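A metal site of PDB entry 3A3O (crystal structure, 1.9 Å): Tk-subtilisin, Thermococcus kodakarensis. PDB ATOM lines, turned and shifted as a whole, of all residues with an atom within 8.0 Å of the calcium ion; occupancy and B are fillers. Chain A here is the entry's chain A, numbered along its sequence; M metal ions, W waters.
OD2 of Asp 310 sits at hydrogen-bond distance from N of Tyr 313 (2.9 Å).
N of Asp 312 is in hydrogen-bond range of OD2 of Asp 310 (3.0 Å).
Five residues have an atom within 4 Å of the calcium ion: Asp 303, Leu 304, Pro 306, Gly 308 and Asp 310.
The calcium ion is bound by OD1 of Asp 303.
O of Leu 304 binds the calcium ion (2.2 Å).
The calcium ion is bound by OD1 of Asp 310 (2.2 Å).
The calcium ion is bound by O of Gly 308 (2.3 Å).
Water W1 binds the calcium ion (2.4 Å).
O of Pro 306 is bound to the calcium ion.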
ATOM      1  N   ASP A 302      25.300  27.699   8.562  1.00  0.00           N
ATOM      2  CA  ASP A 302      25.800  26.579   9.368  1.00  0.00           C
ATOM      3  C   ASP A 302      26.589  25.649   8.420  1.00  0.00           C
ATOM      4  O   ASP A 302      26.019  24.972   7.554  1.00  0.00           O
ATOM      5  CB  ASP A 302      24.649  25.818  10.029  1.00  0.00           C
ATOM      6  CG  ASP A 302      25.137  24.808  11.056  1.00  0.00           C
ATOM      7  OD1 ASP A 302      26.358  24.570  11.130  1.00  0.00           O
ATOM      8  OD2 ASP A 302      24.295  24.255  11.785  1.00  0.00           O
ATOM      9  N   ASP A 303      27.912  25.648   8.583  1.00  0.00           N
ATOM     10  CA  ASP A 303      28.781  24.934   7.672  1.00  0.00           C
ATOM     11  C   ASP A 303      28.758  23.446   7.947  1.00  0.00           C
ATOM     12  O   ASP A 303      29.511  22.927   8.778  1.00  0.00           O
ATOM     13  CB  ASP A 303      30.213  25.486   7.768  1.00  0.00           C
ATOM     14  CG  ASP A 303      31.213  24.736   6.878  1.00  0.00           C
ATOM     15  OD1 ASP A 303      30.810  23.891   6.013  1.00  0.00           O
ATOM     16  OD2 ASP A 303      32.416  24.990   7.070  1.00  0.00           O
ATOM     17  N   LEU A 304      27.906  22.737   7.220  1.00  0.00           N
ATOM     18  CA  LEU A 304      27.843  21.271   7.339  1.00  0.00           C
ATOM     19  C   LEU A 304      28.834  20.575   6.394  1.00  0.00           C
ATOM     20  O   LEU A 304      29.524  21.216   5.583  1.00  0.00           O
ATOM     21  CB  LEU A 304      26.423  20.759   7.135  1.00  0.00           C
ATOM     22  CG  LEU A 304      25.324  21.398   8.027  1.00  0.00           C
ATOM     23  CD1 LEU A 304      23.975  20.760   7.750  1.00  0.00           C
ATOM     24  CD2 LEU A 304      25.633  21.330   9.536  1.00  0.00           C
ATOM     25  N   GLY A 305      28.913  19.256   6.554  1.00  0.00           N
ATOM     26  CA  GLY A 305      29.764  18.395   5.753  1.00  0.00           C
ATOM     27  C   GLY A 305      31.206  18.814   5.925  1.00  0.00           C
ATOM     28  O   GLY A 305      31.564  19.340   6.976  1.00  0.00           O
ATOM     29  N   PRO A 306      32.044  18.588   4.893  1.00  0.00           N
ATOM     30  CA  PRO A 306      33.451  19.047   4.923  1.00  0.00           C
ATOM     31  C   PRO A 306      33.594  20.541   5.184  1.00  0.00           C
ATOM     32  O   PRO A 306      32.767  21.323   4.688  1.00  0.00           O
ATOM     33  CB  PRO A 306      33.927  18.754   3.510  1.00  0.00           C
ATOM     34  CG  PRO A 306      33.096  17.582   3.082  1.00  0.00           C
ATOM     35  CD  PRO A 306      31.731  17.882   3.642  1.00  0.00           C
ATOM     36  N   THR A 307      34.641  20.950   5.896  1.00  0.00           N
ATOM     37  CA  THR A 307      34.895  22.375   6.151  1.00  0.00           C
ATOM     38  C   THR A 307      34.792  23.206   4.875  1.00  0.00           C
ATOM     39  O   THR A 307      35.331  22.834   3.846  1.00  0.00           O
ATOM     40  CB  THR A 307      36.269  22.604   6.848  1.00  0.00           C
ATOM     41  OG1 THR A 307      36.226  22.001   8.137  1.00  0.00           O
ATOM     42  CG2 THR A 307      36.562  24.090   7.025  1.00  0.00           C
ATOM     43  N   GLY A 308      34.061  24.313   4.963  1.00  0.00           N
ATOM     44  CA  GLY A 308      33.955  25.281   3.873  1.00  0.00           C
ATOM     45  C   GLY A 308      32.848  24.940   2.880  1.00  0.00           C
ATOM     46  O   GLY A 308      32.087  23.977   3.068  1.00  0.00           O
ATOM     47  N   TRP A 309      32.778  25.728   1.814  1.00  0.00           N
ATOM     48  CA  TRP A 309      31.851  25.457   0.720  1.00  0.00           C
ATOM     49  C   TRP A 309      32.127  24.061   0.197  1.00  0.00           C
ATOM     50  O   TRP A 309      33.294  23.696  -0.029  1.00  0.00           O
ATOM     51  CB  TRP A 309      32.007  26.492  -0.409  1.00  0.00           C
ATOM     52  CG  TRP A 309      30.997  26.291  -1.515  1.00  0.00           C
ATOM     53  CD1 TRP A 309      29.804  26.963  -1.666  1.00  0.00           C
ATOM     54  CD2 TRP A 309      31.062  25.355  -2.583  1.00  0.00           C
ATOM     55  NE1 TRP A 309      29.132  26.501  -2.767  1.00  0.00           N
ATOM     56  CE2 TRP A 309      29.870  25.503  -3.355  1.00  0.00           C
ATOM     57  CE3 TRP A 309      32.006  24.386  -2.984  1.00  0.00           C
ATOM     58  CZ2 TRP A 309      29.614  24.732  -4.491  1.00  0.00           C
ATOM     59  CZ3 TRP A 309      31.742  23.612  -4.106  1.00  0.00           C
ATOM     60  CH2 TRP A 309      30.567  23.798  -4.864  1.00  0.00           C
ATOM     61  N   ASP A 310      31.069  23.273   0.044  1.00  0.00           N
ATOM     62  CA  ASP A 310      31.182  21.914  -0.505  1.00  0.00           C
ATOM     63  C   ASP A 310      30.046  21.675  -1.523  1.00  0.00           C
ATOM     64  O   ASP A 310      29.041  22.398  -1.493  1.00  0.00           O
ATOM     65  CB  ASP A 310      31.209  20.871   0.622  1.00  0.00           C
ATOM     66  CG  ASP A 310      29.918  20.834   1.429  1.00  0.00           C
ATOM     67  OD1 ASP A 310      29.900  21.476   2.512  1.00  0.00           O
ATOM     68  OD2 ASP A 310      28.952  20.167   0.996  1.00  0.00           O
ATOM     69  N   ALA A 311      30.201  20.697  -2.417  1.00  0.00           N
ATOM     70  CA  ALA A 311      29.195  20.465  -3.466  1.00  0.00           C
ATOM     71  C   ALA A 311      27.831  19.992  -2.969  1.00  0.00           C
ATOM     72  O   ALA A 311      26.862  19.984  -3.722  1.00  0.00           O
ATOM     73  CB  ALA A 311      29.739  19.561  -4.582  1.00  0.00           C
ATOM     74  N   ASP A 312      27.721  19.578  -1.712  1.00  0.00           N
ATOM     75  CA  ASP A 312      26.438  19.140  -1.192  1.00  0.00           C
ATOM     76  C   ASP A 312      25.637  20.321  -0.601  1.00  0.00           C
ATOM     77  O   ASP A 312      24.511  20.579  -1.035  1.00  0.00           O
ATOM     78  CB  ASP A 312      26.618  18.039  -0.139  1.00  0.00           C
ATOM     79  CG  ASP A 312      26.947  16.690  -0.770  1.00  0.00           C
ATOM     80  OD1 ASP A 312      26.632  16.494  -1.958  1.00  0.00           O
ATOM     81  OD2 ASP A 312      27.507  15.832  -0.054  1.00  0.00           O
ATOM     82  N   TYR A 313      26.245  21.038   0.340  1.00  0.00           N
ATOM     83  CA  TYR A 313      25.531  22.039   1.165  1.00  0.00           C
ATOM     84  C   TYR A 313      25.721  23.468   0.692  1.00  0.00           C
ATOM     85  O   TYR A 313      25.136  24.419   1.256  1.00  0.00           O
ATOM     86  CB  TYR A 313      26.041  21.944   2.610  1.00  0.00           C
ATOM     87  CG  TYR A 313      25.693  20.636   3.275  1.00  0.00           C
ATOM     88  CD1 TYR A 313      26.671  19.647   3.484  1.00  0.00           C
ATOM     89  CD2 TYR A 313      24.394  20.378   3.702  1.00  0.00           C
ATOM     90  CE1 TYR A 313      26.354  18.440   4.111  1.00  0.00           C
ATOM     91  CE2 TYR A 313      24.069  19.182   4.327  1.00  0.00           C
ATOM     92  CZ  TYR A 313      25.059  18.213   4.535  1.00  0.00           C
ATOM     93  OH  TYR A 313      24.718  17.042   5.163  1.00  0.00           O
ATOM     94  N   GLY A 314      26.599  23.650  -0.299  1.00  0.00           N
ATOM     95  CA  GLY A 314      27.064  24.991  -0.616  1.00  0.00           C
ATOM     96  C   GLY A 314      27.841  25.523   0.566  1.00  0.00           C
ATOM     97  O   GLY A 314      28.571  24.772   1.213  1.00  0.00           O
ATOM     98  N   TYR A 315      27.660  26.799   0.887  1.00  0.00           N
ATOM     99  CA  TYR A 315      28.289  27.351   2.081  1.00  0.00           C
ATOM    100  C   TYR A 315      27.670  26.793   3.372  1.00  0.00           C
ATOM    101  O   TYR A 315      28.265  26.930   4.438  1.00  0.00           O
ATOM    102  CB  TYR A 315      28.180  28.853   2.082  1.00  0.00           C
ATOM    103  CG  TYR A 315      29.112  29.572   1.153  1.00  0.00           C
ATOM    104  CD1 TYR A 315      28.687  30.020  -0.093  1.00  0.00           C
ATOM    105  CD2 TYR A 315      30.435  29.830   1.529  1.00  0.00           C
ATOM    106  CE1 TYR A 315      29.536  30.727  -0.944  1.00  0.00           C
ATOM    107  CE2 TYR A 315      31.288  30.530   0.713  1.00  0.00           C
ATOM    108  CZ  TYR A 315      30.844  30.975  -0.517  1.00  0.00           C
ATOM    109  OH  TYR A 315      31.710  31.672  -1.312  1.00  0.00           O
ATOM    110  N   GLY A 316      26.472  26.230   3.276  1.00  0.00           N
ATOM    111  CA  GLY A 316      25.798  25.633   4.441  1.00  0.00           C
ATOM    112  C   GLY A 316      24.337  26.023   4.586  1.00  0.00           C
ATOM    113  O   GLY A 316      23.753  26.595   3.663  1.00  0.00           O
ATOM    114  N   VAL A 317      23.745  25.704   5.727  1.00  0.00           N
ATOM    115  CA  VAL A 317      22.329  25.969   5.971  1.00  0.00           C
ATOM    116  C   VAL A 317      22.125  27.396   6.454  1.00  0.00           C
ATOM    117  O   VAL A 317      22.713  27.818   7.445  1.00  0.00           O
ATOM    118  CB  VAL A 317      21.737  24.979   7.007  1.00  0.00           C
ATOM    119  CG1 VAL A 317      20.238  25.289   7.260  1.00  0.00           C
ATOM    120  CG2 VAL A 317      21.913  23.507   6.515  1.00  0.00           C
HETATM  121 CA    CA M   1      30.746  22.540   4.295  1.00  0.00          CA
HETATM  122  O   HOH W   1      28.834  23.888   3.802  1.00  0.00           O
